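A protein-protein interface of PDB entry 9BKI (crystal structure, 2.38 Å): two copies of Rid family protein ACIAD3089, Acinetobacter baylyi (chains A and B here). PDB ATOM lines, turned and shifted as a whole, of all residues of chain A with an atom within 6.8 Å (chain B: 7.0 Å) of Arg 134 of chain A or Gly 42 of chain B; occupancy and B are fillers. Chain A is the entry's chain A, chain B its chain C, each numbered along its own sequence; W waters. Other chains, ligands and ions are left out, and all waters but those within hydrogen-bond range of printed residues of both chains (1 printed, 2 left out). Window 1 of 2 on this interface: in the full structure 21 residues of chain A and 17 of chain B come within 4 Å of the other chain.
Water W1 lies within hydrogen-bond range of O of Met 40 of chain B, NE2 of Gln 96 of chain A and OG1 of Thr 133 of chain A.
The backbone carbonyl oxygen of His 132 of chain A lies within hydrogen-bond range of the backbone NH of Thr 29 of chain B (3.0 Å). The backbone NH of Arg 134 of chain A is in hydrogen-bond range of the side-chain hydroxyl of Ser 41 of chain B (3.1 Å). O of Arg 134 of chain A lies within hydrogen-bond range of N of Gly 42 of chain B (3.0 Å). The backbone NH (N) of Gly 42 of chain B is in hydrogen-bond range of the side-chain hydroxyl (OG1) of Thr 135 of chain A (3.4 Å). ND2 of Asn 151 of chain B lies within hydrogen-bond range of OG1 of Thr 135 of chain A, at 2.8 Å. The side-chain carboxylate (OE1) of Glu 149 of chain B sits close to the backbone carbonyl oxygen (O) of Ser 136 of chain A (3.2 Å).
Of the printed residues of chain B, Asn 98 of chain A touches Asn 151 (3.9 Å). Ala 117 of chain A touches none of the printed residues of chain B. Arg 134 of chain A touches just these residues of chain B: Tyr 28, Ser 41 and Gly 42. Of the printed residues of chain B, Ser 136 of chain A touches Glu 149. Of the printed residues of chain A, Ser 41 of chain B touches Thr 133 and Arg 134. Gly 42 of chain B touches just these residues of chain A: Arg 134 (3.0 Å) and Thr 135 (3.4 Å). Phe 100 of chain B touches none of the printed residues of chain A. Of the printed residues of chain A, Glu 149 of chain B touches Thr 135 (3.3 Å) and Ser 136 (3.2 Å). The nearest residue of chain B that does not touch Arg 134 of chain A is Thr 29 of chain B (4.5 Å). The nearest residue of chain A that does not touch Gly 42 of chain B is Ser 136 of chain A (6.0 Å).
Of the 17 printed residues of chain B, 6 touch a printed residue of chain A. Printed residues of chain B that touch a printed residue of chain A: Tyr 28, Thr 29, Ser 41, Gly 42, Glu 149 and Asn 151. Hydrophobic or aromatic side chains of chain A that line the printed part of chain B: His 132.
NH1 of Arg 134 of chain A sits close to O of Ala 114 of chain A (3.4 Å). NE2 of His 132 of chain A is in hydrogen-bond range of OG of Ser 118 of chain A, at 2.8 Å. NH1 of Arg 134 of chain A lies within hydrogen-bond range of OG of Ser 118 of chain A, at 2.8 Å. The backbone carbonyl oxygen (O) of Thr 29 of chain B lies within hydrogen-bond range of the side-chain hydroxyl (OG) of Ser 41 of chain B (2.5 Å). N of Asn 98 of chain B is in hydrogen-bond range of O of Asn 151 of chain B, 2.9 Å away. The backbone carbonyl oxygen of Glu 149 of chain B is in hydrogen-bond range of the backbone NH of Phe 100 of chain B (2.8 Å).
1 position is printed for both chains.
Among the printed residues, pairs that only touch across the chains: Asn 98 of chain A with Asn 151 of chain B (3.9 Å), His 132 of chain A with Tyr 28 of chain B (3.6 Å), Thr 133 of chain A with Thr 29 of chain B (3.4 Å), Thr 133 of chain A with Ser 41 of chain B (3.3 Å), Arg 134 of chain A with Tyr 28 of chain B (3.3 Å) and Thr 135 of chain A with Glu 149 of chain B (3.3 Å).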
ATOM      1  N   LEU A  95     -27.535 -14.813   5.339  1.00  0.00           N
ATOM      2  CA  LEU A  95     -26.217 -14.559   5.917  1.00  0.00           C
ATOM      3  C   LEU A  95     -25.684 -15.784   6.625  1.00  0.00           C
ATOM      4  O   LEU A  95     -24.477 -16.069   6.559  1.00  0.00           O
ATOM      5  CB  LEU A  95     -26.244 -13.381   6.894  1.00  0.00           C
ATOM      6  CG  LEU A  95     -26.681 -12.058   6.270  1.00  0.00           C
ATOM      7  CD1 LEU A  95     -26.670 -10.953   7.297  1.00  0.00           C
ATOM      8  CD2 LEU A  95     -25.781 -11.733   5.096  1.00  0.00           C
ATOM      9  N   GLN A  96     -26.555 -16.502   7.334  1.00  0.00           N
ATOM     10  CA  GLN A  96     -26.044 -17.583   8.159  1.00  0.00           C
ATOM     11  C   GLN A  96     -27.086 -18.673   8.305  1.00  0.00           C
ATOM     12  O   GLN A  96     -28.259 -18.382   8.516  1.00  0.00           O
ATOM     13  CB  GLN A  96     -25.652 -17.062   9.534  1.00  0.00           C
ATOM     14  CG  GLN A  96     -24.896 -18.047  10.356  1.00  0.00           C
ATOM     15  CD  GLN A  96     -24.730 -17.562  11.773  1.00  0.00           C
ATOM     16  OE1 GLN A  96     -25.719 -17.374  12.489  1.00  0.00           O
ATOM     17  NE2 GLN A  96     -23.485 -17.347  12.189  1.00  0.00           N
ATOM     18  N   MET A  97     -26.643 -19.924   8.216  1.00  0.00           N
ATOM     19  CA  MET A  97     -27.493 -21.085   8.432  1.00  0.00           C
ATOM     20  C   MET A  97     -26.763 -22.046   9.356  1.00  0.00           C
ATOM     21  O   MET A  97     -25.677 -22.504   9.020  1.00  0.00           O
ATOM     22  CB  MET A  97     -27.845 -21.752   7.107  1.00  0.00           C
ATOM     23  CG  MET A  97     -28.703 -22.987   7.257  1.00  0.00           C
ATOM     24  SD  MET A  97     -29.128 -23.698   5.644  1.00  0.00           S
ATOM     25  CE  MET A  97     -27.650 -24.544   5.108  1.00  0.00           C
ATOM     26  N   ASN A  98     -27.349 -22.330  10.520  1.00  0.00           N
ATOM     27  CA  ASN A  98     -26.768 -23.248  11.490  1.00  0.00           C
ATOM     28  C   ASN A  98     -27.610 -24.519  11.512  1.00  0.00           C
ATOM     29  O   ASN A  98     -28.821 -24.462  11.774  1.00  0.00           O
ATOM     30  CB  ASN A  98     -26.715 -22.637  12.882  1.00  0.00           C
ATOM     31  CG  ASN A  98     -25.847 -21.384  12.947  1.00  0.00           C
ATOM     32  OD1 ASN A  98     -24.699 -21.351  12.479  1.00  0.00           O
ATOM     33  ND2 ASN A  98     -26.419 -20.329  13.502  1.00  0.00           N
ATOM     34  N   VAL A  99     -26.949 -25.649  11.268  1.00  0.00           N
ATOM     35  CA  VAL A  99     -27.567 -26.956  11.092  1.00  0.00           C
ATOM     36  C   VAL A  99     -27.108 -27.842  12.247  1.00  0.00           C
ATOM     37  O   VAL A  99     -25.899 -28.062  12.434  1.00  0.00           O
ATOM     38  CB  VAL A  99     -27.183 -27.578   9.735  1.00  0.00           C
ATOM     39  CG1 VAL A  99     -27.901 -28.911   9.525  1.00  0.00           C
ATOM     40  CG2 VAL A  99     -27.448 -26.601   8.566  1.00  0.00           C
ATOM     41  N   GLN A 110     -21.879 -34.734   8.291  1.00  0.00           N
ATOM     42  CA  GLN A 110     -22.687 -33.551   8.575  1.00  0.00           C
ATOM     43  C   GLN A 110     -22.774 -32.626   7.363  1.00  0.00           C
ATOM     44  O   GLN A 110     -23.834 -32.048   7.100  1.00  0.00           O
ATOM     45  CB  GLN A 110     -22.134 -32.800   9.791  1.00  0.00           C
ATOM     46  CG  GLN A 110     -22.296 -33.519  11.141  1.00  0.00           C
ATOM     47  CD  GLN A 110     -21.260 -34.616  11.367  1.00  0.00           C
ATOM     48  OE1 GLN A 110     -20.416 -34.883  10.518  1.00  0.00           O
ATOM     49  NE2 GLN A 110     -21.319 -35.248  12.528  1.00  0.00           N
ATOM     50  N   SER A 111     -21.688 -32.509   6.587  1.00  0.00           N
ATOM     51  CA  SER A 111     -21.711 -31.629   5.421  1.00  0.00           C
ATOM     52  C   SER A 111     -22.718 -32.117   4.403  1.00  0.00           C
ATOM     53  O   SER A 111     -23.430 -31.316   3.778  1.00  0.00           O
ATOM     54  CB  SER A 111     -20.338 -31.560   4.754  1.00  0.00           C
ATOM     55  OG  SER A 111     -19.388 -31.090   5.677  1.00  0.00           O
ATOM     56  N   GLU A 112     -22.774 -33.433   4.202  1.00  0.00           N
ATOM     57  CA  GLU A 112     -23.694 -33.953   3.211  1.00  0.00           C
ATOM     58  C   GLU A 112     -25.142 -33.754   3.654  1.00  0.00           C
ATOM     59  O   GLU A 112     -26.004 -33.441   2.828  1.00  0.00           O
ATOM     60  CB  GLU A 112     -23.364 -35.420   2.904  1.00  0.00           C
ATOM     61  CG  GLU A 112     -22.043 -35.640   2.122  1.00  0.00           C
ATOM     62  CD  GLU A 112     -20.756 -35.561   2.957  1.00  0.00           C
ATOM     63  OE1 GLU A 112     -20.800 -35.486   4.207  1.00  0.00           O
ATOM     64  OE2 GLU A 112     -19.677 -35.541   2.340  1.00  0.00           O
ATOM     65  N   VAL A 113     -25.423 -33.850   4.958  1.00  0.00           N
ATOM     66  CA  VAL A 113     -26.775 -33.528   5.416  1.00  0.00           C
ATOM     67  C   VAL A 113     -27.081 -32.058   5.160  1.00  0.00           C
ATOM     68  O   VAL A 113     -28.115 -31.714   4.578  1.00  0.00           O
ATOM     69  CB  VAL A 113     -26.958 -33.878   6.898  1.00  0.00           C
ATOM     70  CG1 VAL A 113     -28.350 -33.421   7.384  1.00  0.00           C
ATOM     71  CG2 VAL A 113     -26.756 -35.370   7.108  1.00  0.00           C
ATOM     72  N   ALA A 114     -26.154 -31.172   5.541  1.00  0.00           N
ATOM     73  CA  ALA A 114     -26.368 -29.739   5.355  1.00  0.00           C
ATOM     74  C   ALA A 114     -26.554 -29.359   3.881  1.00  0.00           C
ATOM     75  O   ALA A 114     -27.211 -28.352   3.574  1.00  0.00           O
ATOM     76  CB  ALA A 114     -25.191 -28.972   5.966  1.00  0.00           C
ATOM     77  N   ASP A 115     -25.956 -30.125   2.963  1.00  0.00           N
ATOM     78  CA  ASP A 115     -26.184 -29.889   1.538  1.00  0.00           C
ATOM     79  C   ASP A 115     -27.665 -29.995   1.186  1.00  0.00           C
ATOM     80  O   ASP A 115     -28.124 -29.354   0.233  1.00  0.00           O
ATOM     81  CB  ASP A 115     -25.361 -30.870   0.697  1.00  0.00           C
ATOM     82  CG  ASP A 115     -23.854 -30.644   0.834  1.00  0.00           C
ATOM     83  OD1 ASP A 115     -23.440 -29.508   1.152  1.00  0.00           O
ATOM     84  OD2 ASP A 115     -23.078 -31.598   0.594  1.00  0.00           O
ATOM     85  N   GLY A 116     -28.419 -30.812   1.926  1.00  0.00           N
ATOM     86  CA  GLY A 116     -29.854 -30.881   1.707  1.00  0.00           C
ATOM     87  C   GLY A 116     -30.534 -29.532   1.863  1.00  0.00           C
ATOM     88  O   GLY A 116     -31.383 -29.158   1.051  1.00  0.00           O
ATOM     89  N   ALA A 117     -30.108 -28.748   2.854  1.00  0.00           N
ATOM     90  CA  ALA A 117     -30.679 -27.416   3.039  1.00  0.00           C
ATOM     91  C   ALA A 117     -30.131 -26.441   2.008  1.00  0.00           C
ATOM     92  O   ALA A 117     -30.891 -25.657   1.409  1.00  0.00           O
ATOM     93  CB  ALA A 117     -30.360 -26.918   4.444  1.00  0.00           C
ATOM     94  N   SER A 118     -28.805 -26.503   1.787  1.00  0.00           N
ATOM     95  CA  SER A 118     -28.149 -25.583   0.858  1.00  0.00           C
ATOM     96  C   SER A 118     -28.761 -25.662  -0.539  1.00  0.00           C
ATOM     97  O   SER A 118     -29.007 -24.634  -1.181  1.00  0.00           O
ATOM     98  CB  SER A 118     -26.654 -25.894   0.793  1.00  0.00           C
ATOM     99  OG  SER A 118     -26.014 -25.647   2.037  1.00  0.00           O
ATOM    100  N   GLU A 119     -29.054 -26.875  -1.003  1.00  0.00           N
ATOM    101  CA  GLU A 119     -29.558 -27.077  -2.360  1.00  0.00           C
ATOM    102  C   GLU A 119     -30.969 -26.507  -2.536  1.00  0.00           C
ATOM    103  O   GLU A 119     -31.305 -25.997  -3.608  1.00  0.00           O
ATOM    104  CB  GLU A 119     -29.541 -28.569  -2.678  1.00  0.00           C
ATOM    105  CG  GLU A 119     -28.150 -29.124  -2.904  1.00  0.00           C
ATOM    106  CD  GLU A 119     -28.112 -30.640  -2.771  1.00  0.00           C
ATOM    107  OE1 GLU A 119     -27.053 -31.229  -3.097  1.00  0.00           O
ATOM    108  OE2 GLU A 119     -29.145 -31.234  -2.369  1.00  0.00           O
ATOM    109  N   HIS A 132     -24.699 -18.510   1.240  1.00  0.00           N
ATOM    110  CA  HIS A 132     -24.838 -18.485   2.686  1.00  0.00           C
ATOM    111  C   HIS A 132     -23.579 -19.039   3.328  1.00  0.00           C
ATOM    112  O   HIS A 132     -22.887 -19.879   2.745  1.00  0.00           O
ATOM    113  CB  HIS A 132     -26.038 -19.315   3.117  1.00  0.00           C
ATOM    114  CG  HIS A 132     -25.993 -20.721   2.612  1.00  0.00           C
ATOM    115  ND1 HIS A 132     -26.317 -21.054   1.313  1.00  0.00           N
ATOM    116  CD2 HIS A 132     -25.713 -21.887   3.240  1.00  0.00           C
ATOM    117  CE1 HIS A 132     -26.213 -22.362   1.156  1.00  0.00           C
ATOM    118  NE2 HIS A 132     -25.849 -22.891   2.310  1.00  0.00           N
ATOM    119  N   THR A 133     -23.274 -18.534   4.519  1.00  0.00           N
ATOM    120  CA  THR A 133     -22.347 -19.242   5.380  1.00  0.00           C
ATOM    121  C   THR A 133     -23.116 -20.312   6.150  1.00  0.00           C
ATOM    122  O   THR A 133     -24.339 -20.263   6.276  1.00  0.00           O
ATOM    123  CB  THR A 133     -21.646 -18.304   6.353  1.00  0.00           C
ATOM    124  OG1 THR A 133     -22.583 -17.847   7.327  1.00  0.00           O
ATOM    125  CG2 THR A 133     -21.081 -17.125   5.616  1.00  0.00           C
ATOM    126  N   ARG A 134     -22.377 -21.270   6.693  1.00  0.00           N
ATOM    127  CA  ARG A 134     -23.003 -22.468   7.210  1.00  0.00           C
ATOM    128  C   ARG A 134     -22.137 -23.054   8.313  1.00  0.00           C
ATOM    129  O   ARG A 134     -20.907 -23.019   8.232  1.00  0.00           O
ATOM    130  CB  ARG A 134     -23.152 -23.472   6.062  1.00  0.00           C
ATOM    131  CG  ARG A 134     -24.133 -24.552   6.238  1.00  0.00           C
ATOM    132  CD  ARG A 134     -24.209 -25.375   4.959  1.00  0.00           C
ATOM    133  NE  ARG A 134     -23.143 -26.367   4.850  1.00  0.00           N
ATOM    134  CZ  ARG A 134     -23.091 -27.306   3.912  1.00  0.00           C
ATOM    135  NH1 ARG A 134     -24.013 -27.394   2.967  1.00  0.00           N
ATOM    136  NH2 ARG A 134     -22.094 -28.184   3.928  1.00  0.00           N
ATOM    137  N   THR A 135     -22.795 -23.622   9.317  1.00  0.00           N
ATOM    138  CA  THR A 135     -22.173 -24.419  10.363  1.00  0.00           C
ATOM    139  C   THR A 135     -23.028 -25.661  10.517  1.00  0.00           C
ATOM    140  O   THR A 135     -24.255 -25.583  10.403  1.00  0.00           O
ATOM    141  CB  THR A 135     -22.082 -23.661  11.703  1.00  0.00           C
ATOM    142  OG1 THR A 135     -21.335 -22.445  11.533  1.00  0.00           O
ATOM    143  CG2 THR A 135     -21.434 -24.520  12.789  1.00  0.00           C
ATOM    144  N   SER A 136     -22.385 -26.806  10.725  1.00  0.00           N
ATOM    145  CA  SER A 136     -23.079 -28.093  10.732  1.00  0.00           C
ATOM    146  C   SER A 136     -22.439 -28.990  11.781  1.00  0.00           C
ATOM    147  O   SER A 136     -21.297 -29.412  11.608  1.00  0.00           O
ATOM    148  CB  SER A 136     -22.999 -28.734   9.351  1.00  0.00           C
ATOM    149  OG  SER A 136     -23.828 -29.861   9.271  1.00  0.00           O
ATOM    150  N   TYR B  28     -21.270 -24.122  -0.196  1.00  0.00           N
ATOM    151  CA  TYR B  28     -21.538 -22.931   0.598  1.00  0.00           C
ATOM    152  C   TYR B  28     -20.319 -21.986   0.612  1.00  0.00           C
ATOM    153  O   TYR B  28     -19.233 -22.338   0.149  1.00  0.00           O
ATOM    154  CB  TYR B  28     -21.935 -23.326   2.025  1.00  0.00           C
ATOM    155  CG  TYR B  28     -20.811 -23.953   2.809  1.00  0.00           C
ATOM    156  CD1 TYR B  28     -20.617 -25.342   2.817  1.00  0.00           C
ATOM    157  CD2 TYR B  28     -19.935 -23.163   3.548  1.00  0.00           C
ATOM    158  CE1 TYR B  28     -19.565 -25.926   3.553  1.00  0.00           C
ATOM    159  CE2 TYR B  28     -18.892 -23.724   4.266  1.00  0.00           C
ATOM    160  CZ  TYR B  28     -18.711 -25.099   4.269  1.00  0.00           C
ATOM    161  OH  TYR B  28     -17.678 -25.645   4.992  1.00  0.00           O
ATOM    162  N   THR B  29     -20.511 -20.787   1.150  1.00  0.00           N
ATOM    163  CA  THR B  29     -19.494 -19.749   1.150  1.00  0.00           C
ATOM    164  C   THR B  29     -18.831 -19.678   2.520  1.00  0.00           C
ATOM    165  O   THR B  29     -19.498 -19.839   3.552  1.00  0.00           O
ATOM    166  CB  THR B  29     -20.119 -18.395   0.793  1.00  0.00           C
ATOM    167  OG1 THR B  29     -21.102 -18.593  -0.224  1.00  0.00           O
ATOM    168  CG2 THR B  29     -19.074 -17.448   0.258  1.00  0.00           C
ATOM    169  N   SER B  30     -17.522 -19.410   2.531  1.00  0.00           N
ATOM    170  CA  SER B  30     -16.818 -19.359   3.810  1.00  0.00           C
ATOM    171  C   SER B  30     -17.101 -18.065   4.556  1.00  0.00           C
ATOM    172  O   SER B  30     -17.149 -18.075   5.789  1.00  0.00           O
ATOM    173  CB  SER B  30     -15.311 -19.475   3.614  1.00  0.00           C
ATOM    174  OG  SER B  30     -14.906 -18.666   2.535  1.00  0.00           O
ATOM    175  N   MET B  40     -18.729 -15.860   9.200  1.00  0.00           N
ATOM    176  CA  MET B  40     -17.816 -16.888   8.734  1.00  0.00           C
ATOM    177  C   MET B  40     -18.374 -18.265   9.049  1.00  0.00           C
ATOM    178  O   MET B  40     -18.830 -18.507  10.170  1.00  0.00           O
ATOM    179  CB  MET B  40     -16.451 -16.694   9.383  1.00  0.00           C
ATOM    180  CG  MET B  40     -16.015 -15.234   9.322  1.00  0.00           C
ATOM    181  SD  MET B  40     -14.251 -15.046   9.523  1.00  0.00           S
ATOM    182  CE  MET B  40     -13.655 -16.184   8.248  1.00  0.00           C
ATOM    183  N   SER B  41     -18.315 -19.155   8.059  1.00  0.00           N
ATOM    184  CA  SER B  41     -18.722 -20.544   8.213  1.00  0.00           C
ATOM    185  C   SER B  41     -17.881 -21.228   9.277  1.00  0.00           C
ATOM    186  O   SER B  41     -16.768 -20.792   9.602  1.00  0.00           O
ATOM    187  CB  SER B  41     -18.569 -21.291   6.886  1.00  0.00           C
ATOM    188  OG  SER B  41     -19.435 -20.734   5.903  1.00  0.00           O
ATOM    189  N   GLY B  42     -18.431 -22.303   9.837  1.00  0.00           N
ATOM    190  CA  GLY B  42     -17.674 -23.091  10.798  1.00  0.00           C
ATOM    191  C   GLY B  42     -16.400 -23.641  10.178  1.00  0.00           C
ATOM    192  O   GLY B  42     -16.377 -24.046   9.019  1.00  0.00           O
ATOM    193  N   GLN B  43     -15.329 -23.647  10.955  1.00  0.00           N
ATOM    194  CA  GLN B  43     -14.029 -24.114  10.491  1.00  0.00           C
ATOM    195  C   GLN B  43     -13.588 -25.288  11.350  1.00  0.00           C
ATOM    196  O   GLN B  43     -13.424 -25.144  12.568  1.00  0.00           O
ATOM    197  CB  GLN B  43     -13.002 -22.986  10.566  1.00  0.00           C
ATOM    198  CG  GLN B  43     -13.374 -21.773   9.723  1.00  0.00           C
ATOM    199  CD  GLN B  43     -13.428 -22.113   8.235  1.00  0.00           C
ATOM    200  OE1 GLN B  43     -12.663 -22.951   7.750  1.00  0.00           O
ATOM    201  NE2 GLN B  43     -14.328 -21.457   7.506  1.00  0.00           N
ATOM    202  N   ILE B  44     -13.355 -26.430  10.717  1.00  0.00           N
ATOM    203  CA  ILE B  44     -12.793 -27.593  11.395  1.00  0.00           C
ATOM    204  C   ILE B  44     -11.286 -27.499  11.177  1.00  0.00           C
ATOM    205  O   ILE B  44     -10.862 -26.777  10.264  1.00  0.00           O
ATOM    206  CB  ILE B  44     -13.400 -28.897  10.849  1.00  0.00           C
ATOM    207  CG1 ILE B  44     -13.220 -28.983   9.324  1.00  0.00           C
ATOM    208  CG2 ILE B  44     -14.871 -28.970  11.163  1.00  0.00           C
ATOM    209  CD1 ILE B  44     -13.381 -30.372   8.781  1.00  0.00           C
ATOM    210  N   ARG B  46      -8.717 -28.108   9.433  1.00  0.00           N
ATOM    211  CA  ARG B  46      -8.234 -28.653   8.169  1.00  0.00           C
ATOM    212  C   ARG B  46      -7.241 -27.710   7.496  1.00  0.00           C
ATOM    213  O   ARG B  46      -7.529 -26.528   7.281  1.00  0.00           O
ATOM    214  CB  ARG B  46      -9.435 -29.016   7.294  1.00  0.00           C
ATOM    215  CG  ARG B  46     -10.288 -27.870   6.787  1.00  0.00           C
ATOM    216  CD  ARG B  46     -11.336 -28.441   5.837  1.00  0.00           C
ATOM    217  NE  ARG B  46     -12.283 -27.453   5.334  1.00  0.00           N
ATOM    218  CZ  ARG B  46     -12.090 -26.684   4.274  1.00  0.00           C
ATOM    219  NH1 ARG B  46     -10.988 -26.773   3.547  1.00  0.00           N
ATOM    220  NH2 ARG B  46     -13.038 -25.816   3.925  1.00  0.00           N
ATOM    221  N   SER B  73      -8.347 -24.013  13.783  1.00  0.00           N
ATOM    222  CA  SER B  73      -9.605 -23.463  13.277  1.00  0.00           C
ATOM    223  C   SER B  73      -9.588 -21.939  13.280  1.00  0.00           C
ATOM    224  O   SER B  73     -10.006 -21.298  12.297  1.00  0.00           O
ATOM    225  CB  SER B  73     -10.776 -23.992  14.108  1.00  0.00           C
ATOM    226  OG  SER B  73     -10.947 -25.376  13.879  1.00  0.00           O
ATOM    227  N   ARG B  76      -7.467 -20.757  10.455  1.00  0.00           N
ATOM    228  CA  ARG B  76      -8.185 -20.870   9.184  1.00  0.00           C
ATOM    229  C   ARG B  76      -9.067 -19.653   8.950  1.00  0.00           C
ATOM    230  O   ARG B  76      -9.080 -19.072   7.855  1.00  0.00           O
ATOM    231  CB  ARG B  76      -9.062 -22.120   9.185  1.00  0.00           C
ATOM    232  CG  ARG B  76      -8.413 -23.328   8.538  1.00  0.00           C
ATOM    233  CD  ARG B  76      -9.450 -24.431   8.427  1.00  0.00           C
ATOM    234  NE  ARG B  76     -10.348 -24.159   7.309  1.00  0.00           N
ATOM    235  CZ  ARG B  76     -10.020 -24.376   6.046  1.00  0.00           C
ATOM    236  NH1 ARG B  76      -8.858 -24.926   5.726  1.00  0.00           N
ATOM    237  NH2 ARG B  76     -10.872 -24.031   5.081  1.00  0.00           N
ATOM    238  N   ASN B  98     -18.123 -19.036  18.299  1.00  0.00           N
ATOM    239  CA  ASN B  98     -18.825 -20.197  18.821  1.00  0.00           C
ATOM    240  C   ASN B  98     -17.927 -21.401  18.626  1.00  0.00           C
ATOM    241  O   ASN B  98     -17.465 -21.663  17.502  1.00  0.00           O
ATOM    242  CB  ASN B  98     -20.187 -20.395  18.151  1.00  0.00           C
ATOM    243  CG  ASN B  98     -21.133 -19.230  18.420  1.00  0.00           C
ATOM    244  OD1 ASN B  98     -21.249 -18.757  19.551  1.00  0.00           O
ATOM    245  ND2 ASN B  98     -21.809 -18.768  17.391  1.00  0.00           N
ATOM    246  N   PHE B 100     -17.514 -25.435  19.176  1.00  0.00           N
ATOM    247  CA  PHE B 100     -18.192 -26.713  19.335  1.00  0.00           C
ATOM    248  C   PHE B 100     -17.123 -27.789  19.448  1.00  0.00           C
ATOM    249  O   PHE B 100     -16.307 -27.957  18.538  1.00  0.00           O
ATOM    250  CB  PHE B 100     -19.119 -26.995  18.147  1.00  0.00           C
ATOM    251  CG  PHE B 100     -20.170 -25.944  17.923  1.00  0.00           C
ATOM    252  CD1 PHE B 100     -21.370 -25.985  18.618  1.00  0.00           C
ATOM    253  CD2 PHE B 100     -19.965 -24.919  17.004  1.00  0.00           C
ATOM    254  CE1 PHE B 100     -22.360 -25.009  18.399  1.00  0.00           C
ATOM    255  CE2 PHE B 100     -20.936 -23.958  16.781  1.00  0.00           C
ATOM    256  CZ  PHE B 100     -22.139 -23.999  17.482  1.00  0.00           C
ATOM    257  N   GLU B 149     -14.889 -27.404  16.086  1.00  0.00           N
ATOM    258  CA  GLU B 149     -15.375 -26.568  14.991  1.00  0.00           C
ATOM    259  C   GLU B 149     -15.760 -25.198  15.551  1.00  0.00           C
ATOM    260  O   GLU B 149     -16.445 -25.109  16.574  1.00  0.00           O
ATOM    261  CB  GLU B 149     -16.581 -27.203  14.267  1.00  0.00           C
ATOM    262  CG  GLU B 149     -16.953 -26.413  13.003  1.00  0.00           C
ATOM    263  CD  GLU B 149     -18.158 -26.934  12.257  1.00  0.00           C
ATOM    264  OE1 GLU B 149     -18.510 -28.136  12.354  1.00  0.00           O
ATOM    265  OE2 GLU B 149     -18.779 -26.107  11.566  1.00  0.00           O
ATOM    266  N   ILE B 150     -15.363 -24.135  14.859  1.00  0.00           N
ATOM    267  CA  ILE B 150     -15.488 -22.767  15.368  1.00  0.00           C
ATOM    268  C   ILE B 150     -16.043 -21.873  14.274  1.00  0.00           C
ATOM    269  O   ILE B 150     -15.555 -21.899  13.139  1.00  0.00           O
ATOM    270  CB  ILE B 150     -14.136 -22.222  15.850  1.00  0.00           C
ATOM    271  CG1 ILE B 150     -13.466 -23.211  16.818  1.00  0.00           C
ATOM    272  CG2 ILE B 150     -14.306 -20.873  16.491  1.00  0.00           C
ATOM    273  CD1 ILE B 150     -12.200 -22.627  17.510  1.00  0.00           C
ATOM    274  N   ASN B 151     -17.069 -21.093  14.597  1.00  0.00           N
ATOM    275  CA  ASN B 151     -17.488 -20.061  13.655  1.00  0.00           C
ATOM    276  C   ASN B 151     -17.390 -18.689  14.322  1.00  0.00           C
ATOM    277  O   ASN B 151     -17.225 -18.583  15.542  1.00  0.00           O
ATOM    278  CB  ASN B 151     -18.887 -20.322  13.085  1.00  0.00           C
ATOM    279  CG  ASN B 151     -19.977 -20.242  14.119  1.00  0.00           C
ATOM    280  OD1 ASN B 151     -19.897 -19.478  15.082  1.00  0.00           O
ATOM    281  ND2 ASN B 151     -21.038 -21.020  13.906  1.00  0.00           N
ATOM    282  N   PHE B 152     -17.467 -17.632  13.497  1.00  0.00           N
ATOM    283  CA  PHE B 152     -17.188 -16.272  13.945  1.00  0.00           C
ATOM    284  C   PHE B 152     -18.147 -15.265  13.325  1.00  0.00           C
ATOM    285  O   PHE B 152     -18.561 -15.386  12.167  1.00  0.00           O
ATOM    286  CB  PHE B 152     -15.772 -15.793  13.577  1.00  0.00           C
ATOM    287  CG  PHE B 152     -14.679 -16.613  14.146  1.00  0.00           C
ATOM    288  CD1 PHE B 152     -14.268 -17.775  13.524  1.00  0.00           C
ATOM    289  CD2 PHE B 152     -14.035 -16.206  15.287  1.00  0.00           C
ATOM    290  CE1 PHE B 152     -13.242 -18.536  14.058  1.00  0.00           C
ATOM    291  CE2 PHE B 152     -12.999 -16.956  15.821  1.00  0.00           C
ATOM    292  CZ  PHE B 152     -12.603 -18.121  15.199  1.00  0.00           C
HETATM  293  O   HOH W   1     -21.268 -18.136  10.157  1.00  0.00           O
